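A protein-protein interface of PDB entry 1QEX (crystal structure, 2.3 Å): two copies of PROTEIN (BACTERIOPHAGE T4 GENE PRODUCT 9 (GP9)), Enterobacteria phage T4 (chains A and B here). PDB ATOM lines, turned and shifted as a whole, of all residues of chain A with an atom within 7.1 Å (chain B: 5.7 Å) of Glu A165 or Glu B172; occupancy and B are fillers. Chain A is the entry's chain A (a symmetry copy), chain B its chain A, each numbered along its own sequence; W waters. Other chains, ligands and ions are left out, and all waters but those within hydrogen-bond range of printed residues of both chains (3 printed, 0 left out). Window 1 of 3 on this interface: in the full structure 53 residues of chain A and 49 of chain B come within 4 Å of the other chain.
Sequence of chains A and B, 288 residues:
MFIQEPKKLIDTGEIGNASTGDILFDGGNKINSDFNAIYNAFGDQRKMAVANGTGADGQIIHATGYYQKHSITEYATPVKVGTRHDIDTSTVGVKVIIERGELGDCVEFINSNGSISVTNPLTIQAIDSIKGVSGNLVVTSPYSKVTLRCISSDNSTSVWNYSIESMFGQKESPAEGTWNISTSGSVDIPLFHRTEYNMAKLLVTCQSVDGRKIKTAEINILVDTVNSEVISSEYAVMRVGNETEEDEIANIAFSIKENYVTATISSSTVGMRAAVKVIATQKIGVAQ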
ATOM      1  N   PHE A 109       4.978  -4.971  18.383  1.00  0.00           N
ATOM      2  CA  PHE A 109       4.584  -5.431  19.707  1.00  0.00           C
ATOM      3  C   PHE A 109       4.416  -6.940  19.768  1.00  0.00           C
ATOM      4  O   PHE A 109       4.080  -7.582  18.775  1.00  0.00           O
ATOM      5  CB  PHE A 109       3.238  -4.839  20.124  1.00  0.00           C
ATOM      6  CG  PHE A 109       3.131  -3.357  19.964  1.00  0.00           C
ATOM      7  CD1 PHE A 109       3.013  -2.785  18.702  1.00  0.00           C
ATOM      8  CD2 PHE A 109       3.096  -2.530  21.085  1.00  0.00           C
ATOM      9  CE1 PHE A 109       2.857  -1.412  18.553  1.00  0.00           C
ATOM     10  CE2 PHE A 109       2.939  -1.154  20.947  1.00  0.00           C
ATOM     11  CZ  PHE A 109       2.819  -0.594  19.679  1.00  0.00           C
ATOM     12  N   VAL A 139      -6.461  -4.055  20.499  1.00  0.00           N
ATOM     13  CA  VAL A 139      -6.008  -5.432  20.351  1.00  0.00           C
ATOM     14  C   VAL A 139      -6.406  -6.280  21.549  1.00  0.00           C
ATOM     15  O   VAL A 139      -6.070  -5.965  22.692  1.00  0.00           O
ATOM     16  CB  VAL A 139      -4.473  -5.477  20.187  1.00  0.00           C
ATOM     17  CG1 VAL A 139      -3.997  -6.918  20.072  1.00  0.00           C
ATOM     18  CG2 VAL A 139      -4.064  -4.674  18.955  1.00  0.00           C
ATOM     19  N   SER A 141      -6.337  -9.948  21.122  1.00  0.00           N
ATOM     20  CA  SER A 141      -5.847 -11.293  20.844  1.00  0.00           C
ATOM     21  C   SER A 141      -4.617 -11.640  21.677  1.00  0.00           C
ATOM     22  O   SER A 141      -3.548 -11.060  21.489  1.00  0.00           O
ATOM     23  CB  SER A 141      -5.512 -11.431  19.363  1.00  0.00           C
ATOM     24  OG  SER A 141      -4.997 -12.720  19.084  1.00  0.00           O
ATOM     25  N   PRO A 142      -4.752 -12.598  22.604  1.00  0.00           N
ATOM     26  CA  PRO A 142      -3.615 -12.986  23.445  1.00  0.00           C
ATOM     27  C   PRO A 142      -2.471 -13.635  22.668  1.00  0.00           C
ATOM     28  O   PRO A 142      -2.696 -14.313  21.668  1.00  0.00           O
ATOM     29  CB  PRO A 142      -4.249 -13.933  24.467  1.00  0.00           C
ATOM     30  CG  PRO A 142      -5.395 -14.534  23.720  1.00  0.00           C
ATOM     31  CD  PRO A 142      -5.962 -13.360  22.961  1.00  0.00           C
ATOM     32  N   TYR A 143      -1.245 -13.414  23.135  1.00  0.00           N
ATOM     33  CA  TYR A 143      -0.064 -13.985  22.495  1.00  0.00           C
ATOM     34  C   TYR A 143       0.037 -13.566  21.034  1.00  0.00           C
ATOM     35  O   TYR A 143       0.366 -14.370  20.165  1.00  0.00           O
ATOM     36  CB  TYR A 143      -0.108 -15.511  22.572  1.00  0.00           C
ATOM     37  CG  TYR A 143       0.051 -16.073  23.961  1.00  0.00           C
ATOM     38  CD1 TYR A 143       1.236 -15.888  24.675  1.00  0.00           C
ATOM     39  CD2 TYR A 143      -0.966 -16.816  24.552  1.00  0.00           C
ATOM     40  CE1 TYR A 143       1.405 -16.440  25.946  1.00  0.00           C
ATOM     41  CE2 TYR A 143      -0.810 -17.372  25.820  1.00  0.00           C
ATOM     42  CZ  TYR A 143       0.378 -17.181  26.509  1.00  0.00           C
ATOM     43  OH  TYR A 143       0.542 -17.738  27.752  1.00  0.00           O
ATOM     44  N   SER A 144      -0.234 -12.298  20.763  1.00  0.00           N
ATOM     45  CA  SER A 144      -0.185 -11.818  19.397  1.00  0.00           C
ATOM     46  C   SER A 144       1.051 -10.995  19.101  1.00  0.00           C
ATOM     47  O   SER A 144       1.827 -10.658  20.000  1.00  0.00           O
ATOM     48  CB  SER A 144      -1.433 -10.995  19.092  1.00  0.00           C
ATOM     49  OG  SER A 144      -1.605  -9.976  20.058  1.00  0.00           O
ATOM     50  N   LYS A 145       1.229 -10.698  17.818  1.00  0.00           N
ATOM     51  CA  LYS A 145       2.336  -9.886  17.346  1.00  0.00           C
ATOM     52  C   LYS A 145       1.707  -8.800  16.488  1.00  0.00           C
ATOM     53  O   LYS A 145       1.037  -9.087  15.494  1.00  0.00           O
ATOM     54  CB  LYS A 145       3.311 -10.702  16.503  1.00  0.00           C
ATOM     55  CG  LYS A 145       4.482  -9.872  16.005  1.00  0.00           C
ATOM     56  CD  LYS A 145       5.396 -10.665  15.089  1.00  0.00           C
ATOM     57  CE  LYS A 145       6.506  -9.783  14.537  1.00  0.00           C
ATOM     58  NZ  LYS A 145       7.375 -10.524  13.588  1.00  0.00           N
ATOM     59  N   VAL A 146       1.917  -7.551  16.883  1.00  0.00           N
ATOM     60  CA  VAL A 146       1.345  -6.442  16.152  1.00  0.00           C
ATOM     61  C   VAL A 146       2.433  -5.597  15.526  1.00  0.00           C
ATOM     62  O   VAL A 146       3.404  -5.215  16.177  1.00  0.00           O
ATOM     63  CB  VAL A 146       0.456  -5.576  17.082  1.00  0.00           C
ATOM     64  CG1 VAL A 146      -0.232  -4.463  16.282  1.00  0.00           C
ATOM     65  CG2 VAL A 146      -0.583  -6.465  17.758  1.00  0.00           C
ATOM     66  N   THR A 147       2.272  -5.330  14.239  1.00  0.00           N
ATOM     67  CA  THR A 147       3.231  -4.532  13.499  1.00  0.00           C
ATOM     68  C   THR A 147       2.526  -3.312  12.924  1.00  0.00           C
ATOM     69  O   THR A 147       1.511  -3.437  12.237  1.00  0.00           O
ATOM     70  CB  THR A 147       3.848  -5.342  12.343  1.00  0.00           C
ATOM     71  OG1 THR A 147       4.491  -6.506  12.871  1.00  0.00           O
ATOM     72  CG2 THR A 147       4.877  -4.514  11.593  1.00  0.00           C
ATOM     73  N   TYR A 162      -1.747  -1.719   9.843  1.00  0.00           N
ATOM     74  CA  TYR A 162      -1.203  -2.734  10.726  1.00  0.00           C
ATOM     75  C   TYR A 162      -1.512  -4.163  10.322  1.00  0.00           C
ATOM     76  O   TYR A 162      -2.343  -4.434   9.462  1.00  0.00           O
ATOM     77  CB  TYR A 162      -1.749  -2.525  12.135  1.00  0.00           C
ATOM     78  CG  TYR A 162      -3.227  -2.826  12.215  1.00  0.00           C
ATOM     79  CD1 TYR A 162      -4.163  -1.965  11.645  1.00  0.00           C
ATOM     80  CD2 TYR A 162      -3.688  -4.009  12.801  1.00  0.00           C
ATOM     81  CE1 TYR A 162      -5.520  -2.274  11.649  1.00  0.00           C
ATOM     82  CE2 TYR A 162      -5.046  -4.329  12.810  1.00  0.00           C
ATOM     83  CZ  TYR A 162      -5.954  -3.458  12.229  1.00  0.00           C
ATOM     84  OH  TYR A 162      -7.292  -3.774  12.204  1.00  0.00           O
ATOM     85  N   SER A 163      -0.823  -5.071  10.992  1.00  0.00           N
ATOM     86  CA  SER A 163      -1.006  -6.494  10.807  1.00  0.00           C
ATOM     87  C   SER A 163      -0.990  -7.062  12.216  1.00  0.00           C
ATOM     88  O   SER A 163      -0.327  -6.531  13.110  1.00  0.00           O
ATOM     89  CB  SER A 163       0.149  -7.104  10.006  1.00  0.00           C
ATOM     90  OG  SER A 163       1.331  -7.159  10.786  1.00  0.00           O
ATOM     91  N   ILE A 164      -1.730  -8.136  12.416  1.00  0.00           N
ATOM     92  CA  ILE A 164      -1.758  -8.785  13.708  1.00  0.00           C
ATOM     93  C   ILE A 164      -1.729 -10.271  13.414  1.00  0.00           C
ATOM     94  O   ILE A 164      -2.457 -10.758  12.553  1.00  0.00           O
ATOM     95  CB  ILE A 164      -3.016  -8.399  14.503  1.00  0.00           C
ATOM     96  CG1 ILE A 164      -3.060  -9.192  15.807  1.00  0.00           C
ATOM     97  CG2 ILE A 164      -4.250  -8.621  13.662  1.00  0.00           C
ATOM     98  CD1 ILE A 164      -4.259  -8.868  16.661  1.00  0.00           C
ATOM     99  N   GLU A 165      -0.857 -10.981  14.116  1.00  0.00           N
ATOM    100  CA  GLU A 165      -0.708 -12.407  13.906  1.00  0.00           C
ATOM    101  C   GLU A 165      -0.336 -13.124  15.189  1.00  0.00           C
ATOM    102  O   GLU A 165       0.106 -12.507  16.153  1.00  0.00           O
ATOM    103  CB  GLU A 165       0.353 -12.655  12.824  1.00  0.00           C
ATOM    104  CG  GLU A 165       1.589 -11.787  12.965  1.00  0.00           C
ATOM    105  CD  GLU A 165       2.526 -11.868  11.761  1.00  0.00           C
ATOM    106  OE1 GLU A 165       2.287 -12.697  10.859  1.00  0.00           O
ATOM    107  OE2 GLU A 165       3.508 -11.099  11.721  1.00  0.00           O
ATOM    108  N   SER A 166      -0.532 -14.433  15.201  1.00  0.00           N
ATOM    109  CA  SER A 166      -0.219 -15.237  16.371  1.00  0.00           C
ATOM    110  C   SER A 166       1.279 -15.459  16.481  1.00  0.00           C
ATOM    111  O   SER A 166       1.954 -15.699  15.483  1.00  0.00           O
ATOM    112  CB  SER A 166      -0.931 -16.585  16.291  1.00  0.00           C
ATOM    113  OG  SER A 166      -2.333 -16.401  16.260  1.00  0.00           O
ATOM    114  N   MET A 167       1.791 -15.367  17.700  1.00  0.00           N
ATOM    115  CA  MET A 167       3.202 -15.573  17.959  1.00  0.00           C
ATOM    116  C   MET A 167       3.485 -17.062  17.782  1.00  0.00           C
ATOM    117  O   MET A 167       4.534 -17.450  17.264  1.00  0.00           O
ATOM    118  CB  MET A 167       3.544 -15.147  19.394  1.00  0.00           C
ATOM    119  CG  MET A 167       3.375 -13.645  19.684  1.00  0.00           C
ATOM    120  SD  MET A 167       3.536 -13.164  21.458  1.00  0.00           S
ATOM    121  CE  MET A 167       5.278 -13.489  21.729  1.00  0.00           C
ATOM    122  N   PHE A 168       2.521 -17.890  18.180  1.00  0.00           N
ATOM    123  CA  PHE A 168       2.695 -19.337  18.112  1.00  0.00           C
ATOM    124  C   PHE A 168       1.728 -20.075  17.201  1.00  0.00           C
ATOM    125  O   PHE A 168       0.763 -19.501  16.686  1.00  0.00           O
ATOM    126  CB  PHE A 168       2.599 -19.912  19.525  1.00  0.00           C
ATOM    127  CG  PHE A 168       3.410 -19.152  20.533  1.00  0.00           C
ATOM    128  CD1 PHE A 168       4.795 -19.088  20.422  1.00  0.00           C
ATOM    129  CD2 PHE A 168       2.788 -18.456  21.564  1.00  0.00           C
ATOM    130  CE1 PHE A 168       5.552 -18.339  21.321  1.00  0.00           C
ATOM    131  CE2 PHE A 168       3.533 -17.703  22.467  1.00  0.00           C
ATOM    132  CZ  PHE A 168       4.922 -17.643  22.343  1.00  0.00           C
ATOM    133  N   LYS A 171       1.975 -23.202  11.356  1.00  0.00           N
ATOM    134  CA  LYS A 171       1.456 -22.511  10.187  1.00  0.00           C
ATOM    135  C   LYS A 171       2.097 -22.951   8.880  1.00  0.00           C
ATOM    136  O   LYS A 171       1.678 -22.499   7.817  1.00  0.00           O
ATOM    137  CB  LYS A 171       1.690 -21.008  10.347  1.00  0.00           C
ATOM    138  CG  LYS A 171       1.352 -20.461  11.726  1.00  0.00           C
ATOM    139  CD  LYS A 171       1.972 -19.088  11.926  1.00  0.00           C
ATOM    140  CE  LYS A 171       1.721 -18.562  13.330  1.00  0.00           C
ATOM    141  NZ  LYS A 171       2.392 -17.247  13.559  1.00  0.00           N
ATOM    142  N   GLY B 169      -3.020  -6.708   7.701  1.00  0.00           N
ATOM    143  CA  GLY B 169      -4.140  -7.622   7.792  1.00  0.00           C
ATOM    144  C   GLY B 169      -4.233  -8.358   9.117  1.00  0.00           C
ATOM    145  O   GLY B 169      -3.255  -8.460   9.861  1.00  0.00           O
ATOM    146  N   GLN B 170      -5.428  -8.852   9.424  1.00  0.00           N
ATOM    147  CA  GLN B 170      -5.651  -9.617  10.645  1.00  0.00           C
ATOM    148  C   GLN B 170      -5.450 -11.085  10.265  1.00  0.00           C
ATOM    149  O   GLN B 170      -6.275 -11.680   9.565  1.00  0.00           O
ATOM    150  CB  GLN B 170      -7.065  -9.373  11.175  1.00  0.00           C
ATOM    151  CG  GLN B 170      -7.236  -8.013  11.826  1.00  0.00           C
ATOM    152  CD  GLN B 170      -8.613  -7.817  12.432  1.00  0.00           C
ATOM    153  OE1 GLN B 170      -9.544  -7.363  11.757  1.00  0.00           O
ATOM    154  NE2 GLN B 170      -8.753  -8.172  13.713  1.00  0.00           N
ATOM    155  N   LYS B 171      -4.341 -11.654  10.724  1.00  0.00           N
ATOM    156  CA  LYS B 171      -3.989 -13.027  10.403  1.00  0.00           C
ATOM    157  C   LYS B 171      -3.957 -13.950  11.610  1.00  0.00           C
ATOM    158  O   LYS B 171      -3.756 -15.151  11.449  1.00  0.00           O
ATOM    159  CB  LYS B 171      -2.605 -13.052   9.750  1.00  0.00           C
ATOM    160  CG  LYS B 171      -2.387 -11.977   8.696  1.00  0.00           C
ATOM    161  CD  LYS B 171      -0.906 -11.814   8.394  1.00  0.00           C
ATOM    162  CE  LYS B 171      -0.661 -10.683   7.408  1.00  0.00           C
ATOM    163  NZ  LYS B 171       0.798 -10.466   7.165  1.00  0.00           N
ATOM    164  N   GLU B 172      -4.144 -13.402  12.808  1.00  0.00           N
ATOM    165  CA  GLU B 172      -4.079 -14.210  14.027  1.00  0.00           C
ATOM    166  C   GLU B 172      -5.072 -15.346  14.114  1.00  0.00           C
ATOM    167  O   GLU B 172      -6.116 -15.331  13.475  1.00  0.00           O
ATOM    168  CB  GLU B 172      -4.247 -13.348  15.293  1.00  0.00           C
ATOM    169  CG  GLU B 172      -4.480 -11.871  15.055  1.00  0.00           C
ATOM    170  CD  GLU B 172      -5.830 -11.561  14.449  1.00  0.00           C
ATOM    171  OE1 GLU B 172      -6.852 -11.621  15.166  1.00  0.00           O
ATOM    172  OE2 GLU B 172      -5.857 -11.256  13.243  1.00  0.00           O
ATOM    173  N   SER B 173      -4.720 -16.329  14.929  1.00  0.00           N
ATOM    174  CA  SER B 173      -5.565 -17.480  15.182  1.00  0.00           C
ATOM    175  C   SER B 173      -5.934 -17.399  16.661  1.00  0.00           C
ATOM    176  O   SER B 173      -5.064 -17.445  17.530  1.00  0.00           O
ATOM    177  CB  SER B 173      -4.806 -18.770  14.912  1.00  0.00           C
ATOM    178  OG  SER B 173      -5.544 -19.866  15.409  1.00  0.00           O
ATOM    179  N   PRO B 174      -7.226 -17.268  16.966  1.00  0.00           N
ATOM    180  CA  PRO B 174      -7.645 -17.177  18.366  1.00  0.00           C
ATOM    181  C   PRO B 174      -7.544 -18.461  19.176  1.00  0.00           C
ATOM    182  O   PRO B 174      -7.736 -18.440  20.388  1.00  0.00           O
ATOM    183  CB  PRO B 174      -9.080 -16.667  18.265  1.00  0.00           C
ATOM    184  CG  PRO B 174      -9.542 -17.226  16.943  1.00  0.00           C
ATOM    185  CD  PRO B 174      -8.351 -17.000  16.055  1.00  0.00           C
ATOM    186  N   TYR B 197     -14.771 -11.447  16.721  1.00  0.00           N
ATOM    187  CA  TYR B 197     -14.976 -11.801  15.312  1.00  0.00           C
ATOM    188  C   TYR B 197     -16.438 -12.093  15.009  1.00  0.00           C
ATOM    189  O   TYR B 197     -17.184 -12.508  15.892  1.00  0.00           O
ATOM    190  CB  TYR B 197     -14.155 -13.053  14.961  1.00  0.00           C
ATOM    191  CG  TYR B 197     -12.706 -12.951  15.341  1.00  0.00           C
ATOM    192  CD1 TYR B 197     -11.844 -12.097  14.652  1.00  0.00           C
ATOM    193  CD2 TYR B 197     -12.199 -13.672  16.417  1.00  0.00           C
ATOM    194  CE1 TYR B 197     -10.519 -11.960  15.029  1.00  0.00           C
ATOM    195  CE2 TYR B 197     -10.868 -13.545  16.805  1.00  0.00           C
ATOM    196  CZ  TYR B 197     -10.038 -12.687  16.109  1.00  0.00           C
ATOM    197  OH  TYR B 197      -8.728 -12.527  16.503  1.00  0.00           O
ATOM    198  N   VAL B 278      -8.300 -22.739  14.755  1.00  0.00           N
ATOM    199  CA  VAL B 278      -9.040 -21.731  14.000  1.00  0.00           C
ATOM    200  C   VAL B 278      -8.091 -21.268  12.894  1.00  0.00           C
ATOM    201  O   VAL B 278      -7.031 -20.712  13.179  1.00  0.00           O
ATOM    202  CB  VAL B 278      -9.433 -20.513  14.883  1.00  0.00           C
ATOM    203  CG1 VAL B 278     -10.119 -19.443  14.022  1.00  0.00           C
ATOM    204  CG2 VAL B 278     -10.362 -20.950  16.014  1.00  0.00           C
ATOM    205  N   THR B 281     -10.577 -15.957  10.166  1.00  0.00           N
ATOM    206  CA  THR B 281     -11.575 -15.145  10.850  1.00  0.00           C
ATOM    207  C   THR B 281     -11.896 -13.936  10.007  1.00  0.00           C
ATOM    208  O   THR B 281     -11.121 -13.552   9.130  1.00  0.00           O
ATOM    209  CB  THR B 281     -11.094 -14.590  12.205  1.00  0.00           C
ATOM    210  OG1 THR B 281     -10.047 -13.634  11.978  1.00  0.00           O
ATOM    211  CG2 THR B 281     -10.618 -15.718  13.128  1.00  0.00           C
HETATM  212  O   HOH W   1      -0.956 -15.518  12.657  1.00  0.00           O
HETATM  213  O   HOH W   2      -5.140  -4.672   9.158  1.00  0.00           O
HETATM  214  O   HOH W   3      -7.159 -14.020  18.170  1.00  0.00           O
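Position printed for both chains: 171.
Of the 9 printed residues of chain B, 5 touch a printed residue of chain A.
Printed residues of chain A that touch a printed residue of chain B: Ser A141, Tyr A162, Ser A163, Ile A164, Glu A165 and Ser A166.
Hydrophobic or aromatic side chains of chain A within 4 Å of the printed part of chain B: Ile A164.
Along chain A the printed residues that touch a printed residue of chain B span positions 141 to 166.
Among the printed residues, 10 pairs touch across the chains.
Among the printed residues, no Asp or Glu carboxylate lies within 4 Å of a Lys or Arg side-chain nitrogen of the other chain.
Among the printed residues, merely in contact across the chains: Ser A141 with Glu B172, Ser A163 with Gly B169, Ile A164 with Gln B170, Glu A165 with Glu B172 and Ser A166 with Glu B172.
The backbone NH of Thr A147 is in hydrogen-bond range of the backbone carbonyl oxygen of Ser A163 (3.1 Å).
The backbone carbonyl oxygen (O) of Ser A166 lies within hydrogen-bond range of the side-chain amino group (NZ) of Lys A171.
The backbone NH (N) of Lys A145 sits at hydrogen-bond distance from the backbone carbonyl oxygen (O) of Glu A165 (2.7 Å).
The side-chain hydroxyl (OH) of Tyr B197 lies within hydrogen-bond range of the side-chain carboxylate (OE1) of Glu B172 (2.5 Å).
The backbone carbonyl oxygen of Ser A141 is in hydrogen-bond range of the side-chain hydroxyl of Ser A144, at 2.6 Å.
The side-chain hydroxyl (OG) of Ser B173 sits at hydrogen-bond distance from the backbone carbonyl oxygen (O) of Val B278, at 2.8 Å.
N of Glu B172 is in hydrogen-bond range of O of Ile A164 (3.1 Å).
The backbone NH of Ile A164 is in hydrogen-bond range of the backbone carbonyl oxygen of Gly B169, 3.0 Å away.
The backbone carbonyl oxygen (O) of Tyr A162 sits at hydrogen-bond distance from the backbone NH (N) of Gly B169.
The backbone NH (N) of Ser B173 is in hydrogen-bond range of the side-chain hydroxyl (OG) of Ser A166.
N of Lys B171 is in hydrogen-bond range of O of Ile A164, at 2.8 Å.
Water W3 lies within hydrogen-bond range of OG of Ser A141 (2.7 Å) and OH of Tyr B197 (2.7 Å).
Water W1 bridges the backbone NH of Ser A166 (2.8 Å) and the backbone carbonyl oxygen of Lys B171 (3.1 Å).
Water W2 bridges the backbone carbonyl oxygen (O) of Tyr A162 and the backbone NH (N) of Gly B169.
Of the printed residues of chain B, Ser A141 touches Glu B172 (3.9 Å).
Of the printed residues of chain B, Tyr A162 touches Gly B169.
Printed residues of chain B within 4 Å of Ile A164: Gly B169, Gln B170, Lys B171 and Glu B172.
Glu A165 touches one residue of chain B.
Phe A168 touches none of the printed residues of chain B.
Of the printed residues of chain A, Lys B171 touches Ile A164 (2.8 Å).
Glu B172 touches just these residues of chain A: Ser A141 (3.9 Å), Ile A164 (3.1 Å), Glu A165 (3.7 Å) and Ser A166 (3.6 Å).
Of the printed residues of chain A, Ser B173 touches Ser A166 (2.7 Å).
The nearest printed residue of chain A that does not touch Gly B169 is Glu A165 (5.5 Å).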
